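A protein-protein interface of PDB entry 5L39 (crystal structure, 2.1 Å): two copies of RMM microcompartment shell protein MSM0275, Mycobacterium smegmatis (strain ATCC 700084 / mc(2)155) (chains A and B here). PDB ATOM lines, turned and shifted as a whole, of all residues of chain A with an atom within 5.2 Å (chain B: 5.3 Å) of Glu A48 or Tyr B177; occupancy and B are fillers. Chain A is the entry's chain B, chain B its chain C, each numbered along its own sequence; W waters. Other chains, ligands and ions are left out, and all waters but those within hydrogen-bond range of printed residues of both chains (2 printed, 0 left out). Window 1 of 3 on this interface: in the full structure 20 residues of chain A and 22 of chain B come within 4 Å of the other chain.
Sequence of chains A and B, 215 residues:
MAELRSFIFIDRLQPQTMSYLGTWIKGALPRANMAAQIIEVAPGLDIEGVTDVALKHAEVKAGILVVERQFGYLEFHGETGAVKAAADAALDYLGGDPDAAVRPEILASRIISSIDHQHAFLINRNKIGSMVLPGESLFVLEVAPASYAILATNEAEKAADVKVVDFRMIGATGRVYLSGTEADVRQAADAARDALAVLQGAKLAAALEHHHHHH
OE1 of Glu A48 lies within hydrogen-bond range of NE2 of His B119. The side-chain hydroxyl of Tyr B177 lies within hydrogen-bond range of the side-chain carboxylate of Glu A48 (2.8 Å). The backbone carbonyl oxygen of Val A67 sits at hydrogen-bond distance from the guanidinium group of Arg B175 (3.1 Å).
Val B140 touches Leu A45. Leu A45 touches Arg B175. OH of Tyr B177 touches CD1 of Leu A45 (3.2 Å). Ile B112 touches Glu A48 (CD1 to O, 3.9 Å). His B119 touches Thr A51. Asp A52 touches Ile B112. His B119 touches Leu A65 (CD2 to CD2, 3.8 Å). Tyr B177 touches Val A67 (OH to CG2, 3.7 Å).
Water W2 lies within hydrogen-bond range of OE2 of Glu A48 (2.7 Å) and OH of Tyr B177 (3.4 Å). Water W1 bridges ND1 of His B119 (2.8 Å) and OD1 of Asp A52 (2.9 Å).
Glu A48 touches three residues of chain B. Of the printed residues of chain B, Thr A51 touches His B119 (3.96 Å). Of the printed residues of chain A, Ile B112 touches Glu A48 (3.9 Å) and Asp A52 (3.4 Å). Printed residues of chain A within 4 Å of His B119: Glu A48 (2.7 Å), Thr A51 (3.96 Å) and Leu A65 (3.8 Å). Of the printed residues of chain A, Val B140 touches Leu A45. Of the printed residues of chain A, Arg B175 touches Leu A45 and Val A67. Of chain A, only Leu A45 (3.2 Å), Glu A48 (2.8 Å) and Val A67 (3.7 Å) come within 4 Å of Tyr B177.
The side-chain hydroxyl (OG1) of Thr A51 lies within hydrogen-bond range of the backbone carbonyl oxygen (O) of Ile A47 (2.9 Å). The backbone NH (N) of Ile B112 sits at hydrogen-bond distance from the backbone carbonyl oxygen (O) of Leu B138. N of Val B165 sits at hydrogen-bond distance from O of Tyr B177 (2.7 Å). The backbone NH of Tyr B177 is in hydrogen-bond range of the backbone carbonyl oxygen of Asp B166 (2.9 Å).
No position is printed for both chains. Of the 11 pairs that touch across the chains among the printed residues, none has its exchanged pair printed and touching as well.
Printed residues of chain A that touch a printed residue of chain B: Leu A45, Glu A48, Thr A51, Asp A52, Leu A65 and Val A67. Along chain A the printed residues that touch a printed residue of chain B span positions 45 to 67. Among the printed residues, 11 pairs touch across the chains. Among the printed residues, no Asp or Glu carboxylate lies within 4 Å of a Lys or Arg side-chain nitrogen of the other chain.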
ATOM      1  N   GLY A  44      14.022  -8.762  14.631  1.00  0.00           N
ATOM      2  CA  GLY A  44      13.693  -7.360  14.461  1.00  0.00           C
ATOM      3  C   GLY A  44      14.880  -6.412  14.426  1.00  0.00           C
ATOM      4  O   GLY A  44      14.925  -5.510  13.585  1.00  0.00           O
ATOM      5  N   LEU A  45      15.850  -6.617  15.316  1.00  0.00           N
ATOM      6  CA  LEU A  45      16.936  -5.649  15.470  1.00  0.00           C
ATOM      7  C   LEU A  45      17.893  -5.603  14.285  1.00  0.00           C
ATOM      8  O   LEU A  45      18.716  -4.689  14.196  1.00  0.00           O
ATOM      9  CB  LEU A  45      17.738  -5.925  16.744  1.00  0.00           C
ATOM     10  CG  LEU A  45      17.990  -4.646  17.543  1.00  0.00           C
ATOM     11  CD1 LEU A  45      16.669  -4.103  18.052  1.00  0.00           C
ATOM     12  CD2 LEU A  45      18.932  -4.883  18.699  1.00  0.00           C
ATOM     13  N   ASP A  46      17.791  -6.578  13.382  1.00  0.00           N
ATOM     14  CA  ASP A  46      18.571  -6.547  12.141  1.00  0.00           C
ATOM     15  C   ASP A  46      18.215  -5.333  11.288  1.00  0.00           C
ATOM     16  O   ASP A  46      19.014  -4.888  10.458  1.00  0.00           O
ATOM     17  CB  ASP A  46      18.356  -7.820  11.318  1.00  0.00           C
ATOM     18  CG  ASP A  46      19.367  -8.902  11.638  1.00  0.00           C
ATOM     19  OD1 ASP A  46      20.357  -8.609  12.342  1.00  0.00           O
ATOM     20  OD2 ASP A  46      19.177 -10.045  11.173  1.00  0.00           O
ATOM     21  N   ILE A  47      17.016  -4.798  11.494  1.00  0.00           N
ATOM     22  CA  ILE A  47      16.561  -3.665  10.698  1.00  0.00           C
ATOM     23  C   ILE A  47      17.397  -2.409  10.969  1.00  0.00           C
ATOM     24  O   ILE A  47      17.418  -1.488  10.153  1.00  0.00           O
ATOM     25  CB  ILE A  47      15.070  -3.350  10.951  1.00  0.00           C
ATOM     26  CG1 ILE A  47      14.476  -2.614   9.751  1.00  0.00           C
ATOM     27  CG2 ILE A  47      14.879  -2.546  12.227  1.00  0.00           C
ATOM     28  CD1 ILE A  47      14.390  -3.482   8.499  1.00  0.00           C
ATOM     29  N   GLU A  48      18.091  -2.373  12.105  1.00  0.00           N
ATOM     30  CA  GLU A  48      18.927  -1.216  12.418  1.00  0.00           C
ATOM     31  C   GLU A  48      20.093  -1.139  11.442  1.00  0.00           C
ATOM     32  O   GLU A  48      20.434  -0.064  10.955  1.00  0.00           O
ATOM     33  CB  GLU A  48      19.437  -1.272  13.862  1.00  0.00           C
ATOM     34  CG  GLU A  48      18.337  -1.195  14.926  1.00  0.00           C
ATOM     35  CD  GLU A  48      17.616   0.153  14.961  1.00  0.00           C
ATOM     36  OE1 GLU A  48      18.141   1.136  14.398  1.00  0.00           O
ATOM     37  OE2 GLU A  48      16.521   0.232  15.563  1.00  0.00           O
ATOM     38  N   GLY A  49      20.698  -2.285  11.152  1.00  0.00           N
ATOM     39  CA  GLY A  49      21.787  -2.334  10.190  1.00  0.00           C
ATOM     40  C   GLY A  49      21.307  -2.036   8.777  1.00  0.00           C
ATOM     41  O   GLY A  49      22.009  -1.388   8.004  1.00  0.00           O
ATOM     42  N   VAL A  50      20.109  -2.513   8.438  1.00  0.00           N
ATOM     43  CA  VAL A  50      19.513  -2.227   7.134  1.00  0.00           C
ATOM     44  C   VAL A  50      19.296  -0.727   6.947  1.00  0.00           C
ATOM     45  O   VAL A  50      19.552  -0.176   5.871  1.00  0.00           O
ATOM     46  CB  VAL A  50      18.160  -2.945   6.948  1.00  0.00           C
ATOM     47  CG1 VAL A  50      17.544  -2.582   5.585  1.00  0.00           C
ATOM     48  CG2 VAL A  50      18.326  -4.445   7.080  1.00  0.00           C
ATOM     49  N   THR A  51      18.824  -0.077   8.007  1.00  0.00           N
ATOM     50  CA  THR A  51      18.505   1.348   7.988  1.00  0.00           C
ATOM     51  C   THR A  51      19.773   2.172   7.805  1.00  0.00           C
ATOM     52  O   THR A  51      19.791   3.165   7.074  1.00  0.00           O
ATOM     53  CB  THR A  51      17.786   1.773   9.294  1.00  0.00           C
ATOM     54  OG1 THR A  51      16.517   1.110   9.381  1.00  0.00           O
ATOM     55  CG2 THR A  51      17.560   3.277   9.330  1.00  0.00           C
ATOM     56  N   ASP A  52      20.832   1.742   8.479  1.00  0.00           N
ATOM     57  CA  ASP A  52      22.128   2.392   8.380  1.00  0.00           C
ATOM     58  C   ASP A  52      22.617   2.369   6.935  1.00  0.00           C
ATOM     59  O   ASP A  52      22.983   3.403   6.378  1.00  0.00           O
ATOM     60  CB  ASP A  52      23.130   1.709   9.308  1.00  0.00           C
ATOM     61  CG  ASP A  52      24.547   2.232   9.129  1.00  0.00           C
ATOM     62  OD1 ASP A  52      24.774   3.441   9.351  1.00  0.00           O
ATOM     63  OD2 ASP A  52      25.434   1.424   8.783  1.00  0.00           O
ATOM     64  N   LEU A  65      10.801   3.389  11.268  1.00  0.00           N
ATOM     65  CA  LEU A  65      11.790   2.495  11.844  1.00  0.00           C
ATOM     66  C   LEU A  65      11.163   1.903  13.103  1.00  0.00           C
ATOM     67  O   LEU A  65      11.000   2.594  14.106  1.00  0.00           O
ATOM     68  CB  LEU A  65      13.095   3.228  12.164  1.00  0.00           C
ATOM     69  CG  LEU A  65      14.147   2.363  12.863  1.00  0.00           C
ATOM     70  CD1 LEU A  65      14.531   1.179  11.978  1.00  0.00           C
ATOM     71  CD2 LEU A  65      15.384   3.177  13.260  1.00  0.00           C
ATOM     72  N   VAL A  67      10.995  -1.622  15.701  1.00  0.00           N
ATOM     73  CA  VAL A  67      11.275  -2.964  16.191  1.00  0.00           C
ATOM     74  C   VAL A  67      10.164  -3.345  17.165  1.00  0.00           C
ATOM     75  O   VAL A  67      10.172  -2.925  18.322  1.00  0.00           O
ATOM     76  CB  VAL A  67      12.648  -3.059  16.883  1.00  0.00           C
ATOM     77  CG1 VAL A  67      13.007  -4.514  17.132  1.00  0.00           C
ATOM     78  CG2 VAL A  67      13.731  -2.382  16.051  1.00  0.00           C
ATOM     79  N   ILE B 112      27.330   0.098  14.809  1.00  0.00           N
ATOM     80  CA  ILE B 112      27.041   1.041  13.739  1.00  0.00           C
ATOM     81  C   ILE B 112      27.868   2.302  13.946  1.00  0.00           C
ATOM     82  O   ILE B 112      27.575   3.122  14.814  1.00  0.00           O
ATOM     83  CB  ILE B 112      25.548   1.390  13.671  1.00  0.00           C
ATOM     84  CG1 ILE B 112      24.726   0.106  13.518  1.00  0.00           C
ATOM     85  CG2 ILE B 112      25.288   2.339  12.521  1.00  0.00           C
ATOM     86  CD1 ILE B 112      23.231   0.305  13.626  1.00  0.00           C
ATOM     87  N   HIS B 119      18.800   8.557  11.273  1.00  0.00           N
ATOM     88  CA  HIS B 119      18.797   7.352  12.082  1.00  0.00           C
ATOM     89  C   HIS B 119      18.721   7.715  13.564  1.00  0.00           C
ATOM     90  O   HIS B 119      17.977   7.096  14.319  1.00  0.00           O
ATOM     91  CB  HIS B 119      20.033   6.506  11.784  1.00  0.00           C
ATOM     92  CG  HIS B 119      19.880   5.070  12.168  1.00  0.00           C
ATOM     93  ND1 HIS B 119      20.800   4.104  11.821  1.00  0.00           N
ATOM     94  CD2 HIS B 119      18.912   4.434  12.870  1.00  0.00           C
ATOM     95  CE1 HIS B 119      20.404   2.934  12.296  1.00  0.00           C
ATOM     96  NE2 HIS B 119      19.261   3.108  12.933  1.00  0.00           N
ATOM     97  N   ILE B 123      15.668   6.764  16.166  1.00  0.00           N
ATOM     98  CA  ILE B 123      15.940   6.059  17.414  1.00  0.00           C
ATOM     99  C   ILE B 123      15.412   6.863  18.602  1.00  0.00           C
ATOM    100  O   ILE B 123      14.733   6.316  19.475  1.00  0.00           O
ATOM    101  CB  ILE B 123      17.450   5.775  17.587  1.00  0.00           C
ATOM    102  CG1 ILE B 123      17.901   4.740  16.553  1.00  0.00           C
ATOM    103  CG2 ILE B 123      17.748   5.276  19.004  1.00  0.00           C
ATOM    104  CD1 ILE B 123      19.401   4.598  16.418  1.00  0.00           C
ATOM    105  N   LEU B 138      27.133   3.521  17.584  1.00  0.00           N
ATOM    106  CA  LEU B 138      26.044   2.814  18.233  1.00  0.00           C
ATOM    107  C   LEU B 138      26.291   1.309  18.267  1.00  0.00           C
ATOM    108  O   LEU B 138      26.736   0.717  17.274  1.00  0.00           O
ATOM    109  CB  LEU B 138      24.726   3.123  17.513  1.00  0.00           C
ATOM    110  CG  LEU B 138      23.416   2.579  18.073  1.00  0.00           C
ATOM    111  CD1 LEU B 138      22.983   3.371  19.293  1.00  0.00           C
ATOM    112  CD2 LEU B 138      22.344   2.614  16.995  1.00  0.00           C
ATOM    113  N   PHE B 139      26.030   0.700  19.420  1.00  0.00           N
ATOM    114  CA  PHE B 139      25.988  -0.753  19.524  1.00  0.00           C
ATOM    115  C   PHE B 139      24.562  -1.192  19.797  1.00  0.00           C
ATOM    116  O   PHE B 139      23.920  -0.701  20.725  1.00  0.00           O
ATOM    117  CB  PHE B 139      26.911  -1.272  20.628  1.00  0.00           C
ATOM    118  CG  PHE B 139      26.821  -2.765  20.840  1.00  0.00           C
ATOM    119  CD1 PHE B 139      27.178  -3.647  19.828  1.00  0.00           C
ATOM    120  CD2 PHE B 139      26.388  -3.285  22.051  1.00  0.00           C
ATOM    121  CE1 PHE B 139      27.104  -5.018  20.016  1.00  0.00           C
ATOM    122  CE2 PHE B 139      26.307  -4.658  22.247  1.00  0.00           C
ATOM    123  CZ  PHE B 139      26.668  -5.524  21.227  1.00  0.00           C
ATOM    124  N   VAL B 140      24.067  -2.109  18.978  1.00  0.00           N
ATOM    125  CA  VAL B 140      22.737  -2.655  19.180  1.00  0.00           C
ATOM    126  C   VAL B 140      22.848  -4.153  19.391  1.00  0.00           C
ATOM    127  O   VAL B 140      23.738  -4.809  18.853  1.00  0.00           O
ATOM    128  CB  VAL B 140      21.799  -2.344  17.996  1.00  0.00           C
ATOM    129  CG1 VAL B 140      21.672  -0.843  17.826  1.00  0.00           C
ATOM    130  CG2 VAL B 140      22.315  -2.985  16.721  1.00  0.00           C
ATOM    131  N   LYS B 163      26.526   5.585  26.839  1.00  0.00           N
ATOM    132  CA  LYS B 163      25.231   5.901  27.402  1.00  0.00           C
ATOM    133  C   LYS B 163      24.200   4.918  26.894  1.00  0.00           C
ATOM    134  O   LYS B 163      24.230   4.493  25.733  1.00  0.00           O
ATOM    135  CB  LYS B 163      24.813   7.344  27.105  1.00  0.00           C
ATOM    136  CG  LYS B 163      25.210   7.886  25.759  1.00  0.00           C
ATOM    137  CD  LYS B 163      24.825   9.357  25.666  1.00  0.00           C
ATOM    138  CE  LYS B 163      25.392  10.009  24.420  1.00  0.00           C
ATOM    139  NZ  LYS B 163      25.146  11.478  24.400  1.00  0.00           N
ATOM    140  N   VAL B 164      23.309   4.531  27.798  1.00  0.00           N
ATOM    141  CA  VAL B 164      22.220   3.644  27.467  1.00  0.00           C
ATOM    142  C   VAL B 164      21.150   4.456  26.739  1.00  0.00           C
ATOM    143  O   VAL B 164      20.433   5.244  27.348  1.00  0.00           O
ATOM    144  CB  VAL B 164      21.647   2.974  28.728  1.00  0.00           C
ATOM    145  CG1 VAL B 164      20.532   2.005  28.365  1.00  0.00           C
ATOM    146  CG2 VAL B 164      22.755   2.247  29.478  1.00  0.00           C
ATOM    147  N   VAL B 165      21.079   4.284  25.425  1.00  0.00           N
ATOM    148  CA  VAL B 165      20.128   5.026  24.602  1.00  0.00           C
ATOM    149  C   VAL B 165      18.750   4.392  24.683  1.00  0.00           C
ATOM    150  O   VAL B 165      17.736   5.085  24.795  1.00  0.00           O
ATOM    151  CB  VAL B 165      20.581   5.087  23.139  1.00  0.00           C
ATOM    152  CG1 VAL B 165      19.476   5.665  22.258  1.00  0.00           C
ATOM    153  CG2 VAL B 165      21.862   5.912  23.024  1.00  0.00           C
ATOM    154  N   ASP B 166      18.719   3.064  24.644  1.00  0.00           N
ATOM    155  CA  ASP B 166      17.461   2.332  24.727  1.00  0.00           C
ATOM    156  C   ASP B 166      17.692   0.982  25.403  1.00  0.00           C
ATOM    157  O   ASP B 166      18.775   0.400  25.300  1.00  0.00           O
ATOM    158  CB  ASP B 166      16.849   2.150  23.333  1.00  0.00           C
ATOM    159  CG  ASP B 166      15.360   1.835  23.380  1.00  0.00           C
ATOM    160  OD1 ASP B 166      14.737   2.067  24.436  1.00  0.00           O
ATOM    161  OD2 ASP B 166      14.812   1.369  22.356  1.00  0.00           O
ATOM    162  N   PHE B 167      16.669   0.489  26.091  1.00  0.00           N
ATOM    163  CA  PHE B 167      16.791  -0.735  26.867  1.00  0.00           C
ATOM    164  C   PHE B 167      15.425  -1.371  27.099  1.00  0.00           C
ATOM    165  O   PHE B 167      14.523  -0.739  27.638  1.00  0.00           O
ATOM    166  CB  PHE B 167      17.481  -0.441  28.201  1.00  0.00           C
ATOM    167  CG  PHE B 167      17.497  -1.602  29.151  1.00  0.00           C
ATOM    168  CD1 PHE B 167      18.413  -2.629  28.995  1.00  0.00           C
ATOM    169  CD2 PHE B 167      16.604  -1.660  30.208  1.00  0.00           C
ATOM    170  CE1 PHE B 167      18.435  -3.697  29.872  1.00  0.00           C
ATOM    171  CE2 PHE B 167      16.620  -2.728  31.092  1.00  0.00           C
ATOM    172  CZ  PHE B 167      17.538  -3.746  30.923  1.00  0.00           C
ATOM    173  N   ARG B 175      16.483  -5.898  24.180  1.00  0.00           N
ATOM    174  CA  ARG B 175      17.245  -5.028  23.284  1.00  0.00           C
ATOM    175  C   ARG B 175      18.053  -3.990  24.038  1.00  0.00           C
ATOM    176  O   ARG B 175      17.625  -3.472  25.073  1.00  0.00           O
ATOM    177  CB  ARG B 175      16.318  -4.318  22.294  1.00  0.00           C
ATOM    178  CG  ARG B 175      15.538  -5.257  21.397  1.00  0.00           C
ATOM    179  CD  ARG B 175      14.088  -4.852  21.307  1.00  0.00           C
ATOM    180  NE  ARG B 175      13.257  -5.983  20.907  1.00  0.00           N
ATOM    181  CZ  ARG B 175      11.989  -5.879  20.528  1.00  0.00           C
ATOM    182  NH1 ARG B 175      11.404  -4.689  20.487  1.00  0.00           N
ATOM    183  NH2 ARG B 175      11.311  -6.966  20.187  1.00  0.00           N
ATOM    184  N   VAL B 176      19.223  -3.684  23.491  1.00  0.00           N
ATOM    185  CA  VAL B 176      20.133  -2.711  24.064  1.00  0.00           C
ATOM    186  C   VAL B 176      20.701  -1.796  22.984  1.00  0.00           C
ATOM    187  O   VAL B 176      21.248  -2.268  21.987  1.00  0.00           O
ATOM    188  CB  VAL B 176      21.303  -3.392  24.782  1.00  0.00           C
ATOM    189  CG1 VAL B 176      22.084  -2.375  25.574  1.00  0.00           C
ATOM    190  CG2 VAL B 176      20.801  -4.512  25.680  1.00  0.00           C
ATOM    191  N   TYR B 177      20.563  -0.491  23.184  1.00  0.00           N
ATOM    192  CA  TYR B 177      21.191   0.495  22.314  1.00  0.00           C
ATOM    193  C   TYR B 177      22.172   1.305  23.147  1.00  0.00           C
ATOM    194  O   TYR B 177      21.763   2.017  24.064  1.00  0.00           O
ATOM    195  CB  TYR B 177      20.151   1.427  21.677  1.00  0.00           C
ATOM    196  CG  TYR B 177      19.174   0.778  20.722  1.00  0.00           C
ATOM    197  CD1 TYR B 177      18.254  -0.169  21.163  1.00  0.00           C
ATOM    198  CD2 TYR B 177      19.138   1.147  19.384  1.00  0.00           C
ATOM    199  CE1 TYR B 177      17.341  -0.750  20.290  1.00  0.00           C
ATOM    200  CE2 TYR B 177      18.235   0.575  18.503  1.00  0.00           C
ATOM    201  CZ  TYR B 177      17.338  -0.371  18.960  1.00  0.00           C
ATOM    202  OH  TYR B 177      16.435  -0.934  18.083  1.00  0.00           O
ATOM    203  N   LEU B 178      23.463   1.181  22.844  1.00  0.00           N
ATOM    204  CA  LEU B 178      24.482   1.955  23.536  1.00  0.00           C
ATOM    205  C   LEU B 178      25.164   2.903  22.567  1.00  0.00           C
ATOM    206  O   LEU B 178      25.452   2.531  21.430  1.00  0.00           O
ATOM    207  CB  LEU B 178      25.519   1.031  24.182  1.00  0.00           C
ATOM    208  CG  LEU B 178      24.929  -0.097  25.029  1.00  0.00           C
ATOM    209  CD1 LEU B 178      26.027  -1.004  25.555  1.00  0.00           C
ATOM    210  CD2 LEU B 178      24.100   0.474  26.171  1.00  0.00           C
ATOM    211  N   SER B 179      25.426   4.126  23.010  1.00  0.00           N
ATOM    212  CA  SER B 179      26.139   5.078  22.172  1.00  0.00           C
ATOM    213  C   SER B 179      27.353   5.657  22.887  1.00  0.00           C
ATOM    214  O   SER B 179      27.448   5.618  24.116  1.00  0.00           O
ATOM    215  CB  SER B 179      25.213   6.206  21.733  1.00  0.00           C
ATOM    216  OG  SER B 179      24.896   7.048  22.824  1.00  0.00           O
HETATM  217  O   HOH W   1      22.939   5.361  10.577  1.00  0.00           O
HETATM  218  O   HOH W   2      14.906   1.895  17.006  1.00  0.00           O
